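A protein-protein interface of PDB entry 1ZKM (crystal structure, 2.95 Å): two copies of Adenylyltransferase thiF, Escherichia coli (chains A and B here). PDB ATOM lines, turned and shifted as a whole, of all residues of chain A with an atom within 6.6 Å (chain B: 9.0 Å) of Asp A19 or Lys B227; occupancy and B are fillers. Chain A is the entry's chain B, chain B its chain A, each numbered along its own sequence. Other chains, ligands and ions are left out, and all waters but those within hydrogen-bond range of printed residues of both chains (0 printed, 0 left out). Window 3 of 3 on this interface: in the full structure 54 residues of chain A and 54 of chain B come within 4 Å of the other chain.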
ATOM      1  N   GLN A  14      -3.562  10.125  10.500  1.00  0.00           N
ATOM      2  CA  GLN A  14      -4.540  10.221   9.427  1.00  0.00           C
ATOM      3  C   GLN A  14      -4.115   9.291   8.291  1.00  0.00           C
ATOM      4  O   GLN A  14      -4.946   8.655   7.638  1.00  0.00           O
ATOM      5  CB  GLN A  14      -4.619  11.649   8.898  1.00  0.00           C
ATOM      6  CG  GLN A  14      -5.582  12.523   9.629  1.00  0.00           C
ATOM      7  CD  GLN A  14      -5.719  13.872   8.973  1.00  0.00           C
ATOM      8  OE1 GLN A  14      -6.504  14.709   9.418  1.00  0.00           O
ATOM      9  NE2 GLN A  14      -4.953  14.099   7.915  1.00  0.00           N
ATOM     10  N   LEU A  16      -2.239   6.531   8.585  1.00  0.00           N
ATOM     11  CA  LEU A  16      -2.422   5.139   8.950  1.00  0.00           C
ATOM     12  C   LEU A  16      -3.894   4.741   8.910  1.00  0.00           C
ATOM     13  O   LEU A  16      -4.271   3.679   9.404  1.00  0.00           O
ATOM     14  CB  LEU A  16      -1.851   4.875  10.341  1.00  0.00           C
ATOM     15  CG  LEU A  16      -0.328   4.910  10.437  1.00  0.00           C
ATOM     16  CD1 LEU A  16       0.130   4.780  11.883  1.00  0.00           C
ATOM     17  CD2 LEU A  16       0.232   3.787   9.609  1.00  0.00           C
ATOM     18  N   LEU A  17      -4.731   5.596   8.338  1.00  0.00           N
ATOM     19  CA  LEU A  17      -6.162   5.306   8.245  1.00  0.00           C
ATOM     20  C   LEU A  17      -6.532   4.828   6.859  1.00  0.00           C
ATOM     21  O   LEU A  17      -6.342   5.556   5.878  1.00  0.00           O
ATOM     22  CB  LEU A  17      -6.992   6.548   8.546  1.00  0.00           C
ATOM     23  CG  LEU A  17      -7.368   6.861   9.985  1.00  0.00           C
ATOM     24  CD1 LEU A  17      -8.250   8.093   9.972  1.00  0.00           C
ATOM     25  CD2 LEU A  17      -8.102   5.688  10.605  1.00  0.00           C
ATOM     26  N   ASP A  18      -7.087   3.625   6.778  1.00  0.00           N
ATOM     27  CA  ASP A  18      -7.477   3.054   5.495  1.00  0.00           C
ATOM     28  C   ASP A  18      -8.288   4.012   4.646  1.00  0.00           C
ATOM     29  O   ASP A  18      -8.035   4.153   3.451  1.00  0.00           O
ATOM     30  CB  ASP A  18      -8.258   1.763   5.713  1.00  0.00           C
ATOM     31  CG  ASP A  18      -7.369   0.628   6.159  1.00  0.00           C
ATOM     32  OD1 ASP A  18      -6.517   0.203   5.353  1.00  0.00           O
ATOM     33  OD2 ASP A  18      -7.512   0.173   7.315  1.00  0.00           O
ATOM     34  N   ASP A  19      -9.249   4.686   5.270  1.00  0.00           N
ATOM     35  CA  ASP A  19     -10.107   5.626   4.558  1.00  0.00           C
ATOM     36  C   ASP A  19      -9.444   6.925   4.111  1.00  0.00           C
ATOM     37  O   ASP A  19     -10.117   7.793   3.558  1.00  0.00           O
ATOM     38  CB  ASP A  19     -11.315   5.965   5.416  1.00  0.00           C
ATOM     39  CG  ASP A  19     -12.173   4.763   5.702  1.00  0.00           C
ATOM     40  OD1 ASP A  19     -12.788   4.245   4.743  1.00  0.00           O
ATOM     41  OD2 ASP A  19     -12.223   4.336   6.880  1.00  0.00           O
ATOM     42  N   ILE A  20      -8.143   7.079   4.345  1.00  0.00           N
ATOM     43  CA  ILE A  20      -7.462   8.298   3.931  1.00  0.00           C
ATOM     44  C   ILE A  20      -6.093   8.000   3.336  1.00  0.00           C
ATOM     45  O   ILE A  20      -5.844   8.313   2.173  1.00  0.00           O
ATOM     46  CB  ILE A  20      -7.309   9.296   5.121  1.00  0.00           C
ATOM     47  CG1 ILE A  20      -8.684   9.582   5.742  1.00  0.00           C
ATOM     48  CG2 ILE A  20      -6.723  10.625   4.637  1.00  0.00           C
ATOM     49  CD1 ILE A  20      -8.641  10.355   7.047  1.00  0.00           C
ATOM     50  N   ALA A  21      -5.216   7.386   4.130  1.00  0.00           N
ATOM     51  CA  ALA A  21      -3.850   7.060   3.699  1.00  0.00           C
ATOM     52  C   ALA A  21      -3.162   8.224   2.984  1.00  0.00           C
ATOM     53  O   ALA A  21      -3.594   9.379   3.073  1.00  0.00           O
ATOM     54  CB  ALA A  21      -3.856   5.840   2.793  1.00  0.00           C
ATOM     55  N   GLY A  24      -5.426  10.180   0.436  1.00  0.00           N
ATOM     56  CA  GLY A  24      -6.242  11.258   0.973  1.00  0.00           C
ATOM     57  C   GLY A  24      -5.456  12.397   1.597  1.00  0.00           C
ATOM     58  O   GLY A  24      -5.795  13.578   1.418  1.00  0.00           O
ATOM     59  N   LEU A 205     -15.357  17.833  10.045  1.00  0.00           N
ATOM     60  CA  LEU A 205     -15.464  16.420   9.724  1.00  0.00           C
ATOM     61  C   LEU A 205     -16.030  16.256   8.330  1.00  0.00           C
ATOM     62  O   LEU A 205     -15.496  15.503   7.533  1.00  0.00           O
ATOM     63  CB  LEU A 205     -16.374  15.703  10.719  1.00  0.00           C
ATOM     64  CG  LEU A 205     -16.573  14.201  10.473  1.00  0.00           C
ATOM     65  CD1 LEU A 205     -15.297  13.456  10.813  1.00  0.00           C
ATOM     66  CD2 LEU A 205     -17.697  13.670  11.337  1.00  0.00           C
ATOM     67  N   GLU A 206     -17.108  16.967   8.029  1.00  0.00           N
ATOM     68  CA  GLU A 206     -17.716  16.851   6.713  1.00  0.00           C
ATOM     69  C   GLU A 206     -16.802  17.356   5.604  1.00  0.00           C
ATOM     70  O   GLU A 206     -16.801  16.805   4.501  1.00  0.00           O
ATOM     71  CB  GLU A 206     -19.051  17.598   6.657  1.00  0.00           C
ATOM     72  CG  GLU A 206     -20.139  17.036   7.557  1.00  0.00           C
ATOM     73  CD  GLU A 206     -20.255  15.525   7.467  1.00  0.00           C
ATOM     74  OE1 GLU A 206     -20.183  14.993   6.344  1.00  0.00           O
ATOM     75  OE2 GLU A 206     -20.423  14.869   8.519  1.00  0.00           O
ATOM     76  N   LYS A 209     -14.196  14.731   4.961  1.00  0.00           N
ATOM     77  CA  LYS A 209     -14.810  13.605   4.265  1.00  0.00           C
ATOM     78  C   LYS A 209     -15.101  13.986   2.814  1.00  0.00           C
ATOM     79  O   LYS A 209     -15.047  13.150   1.915  1.00  0.00           O
ATOM     80  CB  LYS A 209     -16.110  13.184   4.964  1.00  0.00           C
ATOM     81  CG  LYS A 209     -15.876  12.292   6.179  1.00  0.00           C
ATOM     82  CD  LYS A 209     -17.053  12.284   7.153  1.00  0.00           C
ATOM     83  CE  LYS A 209     -18.277  11.635   6.565  1.00  0.00           C
ATOM     84  NZ  LYS A 209     -19.450  11.750   7.468  1.00  0.00           N
ATOM     85  N   SER A 212     -11.529  14.333   1.072  1.00  0.00           N
ATOM     86  CA  SER A 212     -10.761  13.099   0.948  1.00  0.00           C
ATOM     87  C   SER A 212     -11.505  12.119   0.037  1.00  0.00           C
ATOM     88  O   SER A 212     -10.905  11.213  -0.539  1.00  0.00           O
ATOM     89  CB  SER A 212     -10.506  12.473   2.324  1.00  0.00           C
ATOM     90  OG  SER A 212     -11.527  11.560   2.679  1.00  0.00           O
ATOM     91  N   GLY A 213     -12.812  12.307  -0.095  1.00  0.00           N
ATOM     92  CA  GLY A 213     -13.597  11.451  -0.963  1.00  0.00           C
ATOM     93  C   GLY A 213     -14.381  10.345  -0.286  1.00  0.00           C
ATOM     94  O   GLY A 213     -14.646   9.304  -0.883  1.00  0.00           O
ATOM     95  N   ILE A 214     -14.779  10.564   0.956  1.00  0.00           N
ATOM     96  CA  ILE A 214     -15.525   9.551   1.674  1.00  0.00           C
ATOM     97  C   ILE A 214     -17.026   9.791   1.539  1.00  0.00           C
ATOM     98  O   ILE A 214     -17.471  10.935   1.565  1.00  0.00           O
ATOM     99  CB  ILE A 214     -15.089   9.560   3.134  1.00  0.00           C
ATOM    100  CG1 ILE A 214     -13.563   9.490   3.178  1.00  0.00           C
ATOM    101  CG2 ILE A 214     -15.692   8.380   3.890  1.00  0.00           C
ATOM    102  CD1 ILE A 214     -12.990   9.408   4.564  1.00  0.00           C
ATOM    103  N   GLU A 215     -17.794   8.713   1.373  1.00  0.00           N
ATOM    104  CA  GLU A 215     -19.254   8.783   1.214  1.00  0.00           C
ATOM    105  C   GLU A 215     -19.927   9.402   2.434  1.00  0.00           C
ATOM    106  O   GLU A 215     -19.636   9.016   3.563  1.00  0.00           O
ATOM    107  CB  GLU A 215     -19.825   7.379   0.997  1.00  0.00           C
ATOM    108  CG  GLU A 215     -19.157   6.594  -0.121  1.00  0.00           C
ATOM    109  CD  GLU A 215     -19.615   5.146  -0.173  1.00  0.00           C
ATOM    110  OE1 GLU A 215     -19.467   4.437   0.847  1.00  0.00           O
ATOM    111  OE2 GLU A 215     -20.119   4.718  -1.235  1.00  0.00           O
ATOM    112  N   THR A 216     -20.843  10.342   2.217  1.00  0.00           N
ATOM    113  CA  THR A 216     -21.504  10.976   3.351  1.00  0.00           C
ATOM    114  C   THR A 216     -22.947  11.410   3.137  1.00  0.00           C
ATOM    115  O   THR A 216     -23.191  12.457   2.541  1.00  0.00           O
ATOM    116  CB  THR A 216     -20.750  12.230   3.796  1.00  0.00           C
ATOM    117  OG1 THR A 216     -19.363  11.924   3.959  1.00  0.00           O
ATOM    118  CG2 THR A 216     -21.320  12.744   5.112  1.00  0.00           C
ATOM    119  N   PRO A 217     -23.922  10.625   3.633  1.00  0.00           N
ATOM    120  CA  PRO A 217     -25.312  11.053   3.436  1.00  0.00           C
ATOM    121  C   PRO A 217     -25.344  12.548   3.759  1.00  0.00           C
ATOM    122  O   PRO A 217     -24.914  12.963   4.838  1.00  0.00           O
ATOM    123  CB  PRO A 217     -26.073  10.205   4.449  1.00  0.00           C
ATOM    124  CG  PRO A 217     -25.299   8.910   4.420  1.00  0.00           C
ATOM    125  CD  PRO A 217     -23.852   9.381   4.423  1.00  0.00           C
ATOM    126  N   VAL B 154     -11.679   5.877  17.860  1.00  0.00           N
ATOM    127  CA  VAL B 154     -10.717   5.143  17.036  1.00  0.00           C
ATOM    128  C   VAL B 154     -11.138   5.323  15.587  1.00  0.00           C
ATOM    129  O   VAL B 154     -12.277   5.033  15.226  1.00  0.00           O
ATOM    130  CB  VAL B 154     -10.705   3.631  17.336  1.00  0.00           C
ATOM    131  CG1 VAL B 154      -9.517   3.006  16.652  1.00  0.00           C
ATOM    132  CG2 VAL B 154     -10.638   3.377  18.829  1.00  0.00           C
ATOM    133  N   GLY B 155     -10.231   5.812  14.758  1.00  0.00           N
ATOM    134  CA  GLY B 155     -10.588   6.012  13.370  1.00  0.00           C
ATOM    135  C   GLY B 155     -11.725   7.009  13.195  1.00  0.00           C
ATOM    136  O   GLY B 155     -11.536   8.205  13.443  1.00  0.00           O
ATOM    137  N   PHE B 156     -12.892   6.527  12.761  1.00  0.00           N
ATOM    138  CA  PHE B 156     -14.066   7.381  12.548  1.00  0.00           C
ATOM    139  C   PHE B 156     -15.140   7.062  13.572  1.00  0.00           C
ATOM    140  O   PHE B 156     -16.309   7.448  13.407  1.00  0.00           O
ATOM    141  CB  PHE B 156     -14.693   7.151  11.166  1.00  0.00           C
ATOM    142  CG  PHE B 156     -13.935   7.757  10.030  1.00  0.00           C
ATOM    143  CD1 PHE B 156     -12.792   7.154   9.537  1.00  0.00           C
ATOM    144  CD2 PHE B 156     -14.389   8.931   9.429  1.00  0.00           C
ATOM    145  CE1 PHE B 156     -12.111   7.710   8.452  1.00  0.00           C
ATOM    146  CE2 PHE B 156     -13.719   9.494   8.348  1.00  0.00           C
ATOM    147  CZ  PHE B 156     -12.578   8.881   7.857  1.00  0.00           C
ATOM    148  N   GLY B 157     -14.764   6.365  14.632  1.00  0.00           N
ATOM    149  CA  GLY B 157     -15.782   6.000  15.593  1.00  0.00           C
ATOM    150  C   GLY B 157     -15.635   6.585  16.971  1.00  0.00           C
ATOM    151  O   GLY B 157     -14.530   6.640  17.530  1.00  0.00           O
ATOM    152  N   GLY B 158     -16.765   7.001  17.532  1.00  0.00           N
ATOM    153  CA  GLY B 158     -16.742   7.590  18.848  1.00  0.00           C
ATOM    154  C   GLY B 158     -17.685   6.913  19.809  1.00  0.00           C
ATOM    155  O   GLY B 158     -18.752   6.416  19.430  1.00  0.00           O
ATOM    156  N   ARG B 187      -8.025  -1.421  13.849  1.00  0.00           N
ATOM    157  CA  ARG B 187      -7.870  -0.080  13.290  1.00  0.00           C
ATOM    158  C   ARG B 187      -7.309   0.942  14.274  1.00  0.00           C
ATOM    159  O   ARG B 187      -7.233   2.127  13.947  1.00  0.00           O
ATOM    160  CB  ARG B 187      -9.217   0.419  12.754  1.00  0.00           C
ATOM    161  CG  ARG B 187     -10.363   0.235  13.730  1.00  0.00           C
ATOM    162  CD  ARG B 187     -11.658   0.816  13.199  1.00  0.00           C
ATOM    163  NE  ARG B 187     -12.794   0.420  14.029  1.00  0.00           N
ATOM    164  CZ  ARG B 187     -14.043   0.834  13.839  1.00  0.00           C
ATOM    165  NH1 ARG B 187     -14.329   1.668  12.845  1.00  0.00           N
ATOM    166  NH2 ARG B 187     -15.009   0.406  14.643  1.00  0.00           N
ATOM    167  N   VAL B 192      -9.527  10.227  13.189  1.00  0.00           N
ATOM    168  CA  VAL B 192      -9.898  11.492  12.573  1.00  0.00           C
ATOM    169  C   VAL B 192     -10.047  12.520  13.685  1.00  0.00           C
ATOM    170  O   VAL B 192     -10.712  12.247  14.691  1.00  0.00           O
ATOM    171  CB  VAL B 192     -11.226  11.375  11.833  1.00  0.00           C
ATOM    172  CG1 VAL B 192     -11.661  12.730  11.340  1.00  0.00           C
ATOM    173  CG2 VAL B 192     -11.083  10.419  10.679  1.00  0.00           C
ATOM    174  N   VAL B 195     -13.526  13.558  14.835  1.00  0.00           N
ATOM    175  CA  VAL B 195     -14.226  12.516  15.558  1.00  0.00           C
ATOM    176  C   VAL B 195     -13.844  12.502  17.025  1.00  0.00           C
ATOM    177  O   VAL B 195     -14.697  12.645  17.895  1.00  0.00           O
ATOM    178  CB  VAL B 195     -13.985  11.131  14.937  1.00  0.00           C
ATOM    179  CG1 VAL B 195     -14.519  10.035  15.871  1.00  0.00           C
ATOM    180  CG2 VAL B 195     -14.689  11.059  13.573  1.00  0.00           C
ATOM    181  N   PHE B 224     -20.905   7.110  17.885  1.00  0.00           N
ATOM    182  CA  PHE B 224     -20.866   7.965  16.721  1.00  0.00           C
ATOM    183  C   PHE B 224     -20.105   7.331  15.563  1.00  0.00           C
ATOM    184  O   PHE B 224     -19.012   6.780  15.727  1.00  0.00           O
ATOM    185  CB  PHE B 224     -20.257   9.325  17.086  1.00  0.00           C
ATOM    186  CG  PHE B 224     -20.186  10.291  15.927  1.00  0.00           C
ATOM    187  CD1 PHE B 224     -21.294  10.511  15.116  1.00  0.00           C
ATOM    188  CD2 PHE B 224     -19.007  10.966  15.639  1.00  0.00           C
ATOM    189  CE1 PHE B 224     -21.224  11.393  14.027  1.00  0.00           C
ATOM    190  CE2 PHE B 224     -18.928  11.842  14.563  1.00  0.00           C
ATOM    191  CZ  PHE B 224     -20.037  12.058  13.753  1.00  0.00           C
ATOM    192  N   ASP B 225     -20.698   7.398  14.383  1.00  0.00           N
ATOM    193  CA  ASP B 225     -20.050   6.856  13.213  1.00  0.00           C
ATOM    194  C   ASP B 225     -19.654   8.035  12.329  1.00  0.00           C
ATOM    195  O   ASP B 225     -20.439   8.503  11.502  1.00  0.00           O
ATOM    196  CB  ASP B 225     -20.997   5.930  12.455  1.00  0.00           C
ATOM    197  CG  ASP B 225     -20.286   5.105  11.402  1.00  0.00           C
ATOM    198  OD1 ASP B 225     -20.977   4.372  10.662  1.00  0.00           O
ATOM    199  OD2 ASP B 225     -19.044   5.179  11.320  1.00  0.00           O
ATOM    200  N   GLY B 226     -18.433   8.519  12.517  1.00  0.00           N
ATOM    201  CA  GLY B 226     -17.977   9.635  11.721  1.00  0.00           C
ATOM    202  C   GLY B 226     -18.122   9.401  10.230  1.00  0.00           C
ATOM    203  O   GLY B 226     -18.329  10.354   9.476  1.00  0.00           O
ATOM    204  N   LYS B 227     -18.012   8.145   9.793  1.00  0.00           N
ATOM    205  CA  LYS B 227     -18.123   7.830   8.366  1.00  0.00           C
ATOM    206  C   LYS B 227     -19.531   8.045   7.837  1.00  0.00           C
ATOM    207  O   LYS B 227     -19.724   8.772   6.862  1.00  0.00           O
ATOM    208  CB  LYS B 227     -17.674   6.391   8.074  1.00  0.00           C
ATOM    209  CG  LYS B 227     -16.330   6.315   7.348  1.00  0.00           C
ATOM    210  CD  LYS B 227     -16.184   5.039   6.512  1.00  0.00           C
ATOM    211  CE  LYS B 227     -16.010   3.773   7.367  1.00  0.00           C
ATOM    212  NZ  LYS B 227     -14.648   3.628   7.992  1.00  0.00           N
ATOM    213  N   SER B 228     -20.517   7.425   8.477  1.00  0.00           N
ATOM    214  CA  SER B 228     -21.892   7.592   8.033  1.00  0.00           C
ATOM    215  C   SER B 228     -22.537   8.829   8.663  1.00  0.00           C
ATOM    216  O   SER B 228     -23.644   9.217   8.295  1.00  0.00           O
ATOM    217  CB  SER B 228     -22.714   6.349   8.377  1.00  0.00           C
ATOM    218  OG  SER B 228     -22.875   6.209   9.776  1.00  0.00           O
ATOM    219  N   SER B 229     -21.834   9.456   9.599  1.00  0.00           N
ATOM    220  CA  SER B 229     -22.351  10.631  10.292  1.00  0.00           C
ATOM    221  C   SER B 229     -23.683  10.301  10.942  1.00  0.00           C
ATOM    222  O   SER B 229     -24.639  11.073  10.864  1.00  0.00           O
ATOM    223  CB  SER B 229     -22.512  11.808   9.334  1.00  0.00           C
ATOM    224  OG  SER B 229     -21.287  12.505   9.190  1.00  0.00           O
ATOM    225  N   GLN B 230     -23.727   9.139  11.585  1.00  0.00           N
ATOM    226  CA  GLN B 230     -24.922   8.678  12.263  1.00  0.00           C
ATOM    227  C   GLN B 230     -24.716   8.444  13.750  1.00  0.00           C
ATOM    228  O   GLN B 230     -23.678   7.936  14.184  1.00  0.00           O
ATOM    229  CB  GLN B 230     -25.429   7.404  11.598  1.00  0.00           C
ATOM    230  CG  GLN B 230     -26.191   7.713  10.345  1.00  0.00           C
ATOM    231  CD  GLN B 230     -27.033   8.956  10.535  1.00  0.00           C
ATOM    232  OE1 GLN B 230     -27.765   9.077  11.524  1.00  0.00           O
ATOM    233  NE2 GLN B 230     -26.928   9.895   9.598  1.00  0.00           N
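Of the printed residues of chain B, Asp A19 touches Phe B156 (3.6 Å) and Lys B227 (2.8 Å).
Of the printed residues of chain A, Lys B227 touches Asp A19, Lys A209 and Glu A215.
Printed residues of chain B within 4 Å of Glu A215: Lys B227.
Of the printed residues of chain A, Phe B224 touches Leu A205 (3.7 Å).
Printed residues of chain B within 4 Å of Leu A17: Gly B155 and Val B192.
The nearest residue of chain A that does not touch Lys B227 is Ile A214 (4.1 Å).
The nearest printed residue of chain B that does not touch Leu A17 is Phe B156 (4.2 Å).
No position is printed for both chains.
Of the 15 printed residues of chain B, 9 touch a printed residue of chain A.
Printed residues of chain B that touch a printed residue of chain A: Gly B155, Phe B156, Val B192, Val B195, Phe B224, Gly B226, Lys B227, Ser B228 and Ser B229.
Along chain B the printed residues that touch a printed residue of chain A span positions 155 to 229.
Printed residues of chain A that touch a printed residue of chain B: Leu A17, Asp A19, Leu A205, Glu A206, Lys A209, Ile A214, Glu A215 and Pro A217.
Hydrophobic or aromatic side chains of chain A that line the printed part of chain B: Leu A17, Leu A205, Ile A214 and Pro A217.
Among the printed residues, Asp or Glu carboxylates within 4 Å of a Lys or Arg side-chain nitrogen of the other chain: Asp A19 with Lys B227 (2.8 Å).
O of Gly B155 sits at hydrogen-bond distance from N of Val B192 (2.9 Å).
The backbone carbonyl oxygen of Phe B156 lies within hydrogen-bond range of the backbone NH of Gly B226.
N of Phe B224 lies within hydrogen-bond range of O of Gly B158 (2.7 Å).
N of Lys B227 lies close to OD2 of Asp B225.
The side-chain carboxylate (OD1) of Asp B225 sits at hydrogen-bond distance from the side-chain hydroxyl (OG) of Ser B228 (2.8 Å).
O of Ile A214 is in hydrogen-bond range of OG1 of Thr A216.
Leu A17 touches Gly B155.
Val B192 touches Leu A17 (CG2 to CD1, 3.7 Å).
CB of Asp A19 touches CE1 of Phe B156, 3.6 Å away.
CG1 of Val B192 touches CD1 of Leu A205 (3.7 Å).
Leu A205 touches Val B195 (CD1 to CG2, 3.7 Å).
CZ of Phe B224 touches CD2 of Leu A205 (3.7 Å).
CD2 of Leu A205 touches O of Gly B226, 3.9 Å away.
Ile A214 touches Phe B156 (CD1 to CZ, 3.4 Å).
Pro A217 touches Ser B228.
O of Gly B226 lies within hydrogen-bond range of NZ of Lys A209 (2.7 Å).
NZ of Lys B227 is in salt-bridge range of OD2 of Asp A19 (2.8 Å).
NZ of Lys A209 sits at hydrogen-bond distance from O of Lys B227 (3.1 Å).
The side-chain hydroxyl (OG) of Ser B229 lies within hydrogen-bond range of the side-chain carboxylate (OE2) of Glu A206.
The side-chain hydroxyl (OG) of Ser B229 sits at hydrogen-bond distance from the side-chain amino group (NZ) of Lys A209.
The backbone carbonyl oxygen of Glu A215 sits close to the backbone carbonyl oxygen of Lys B227.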
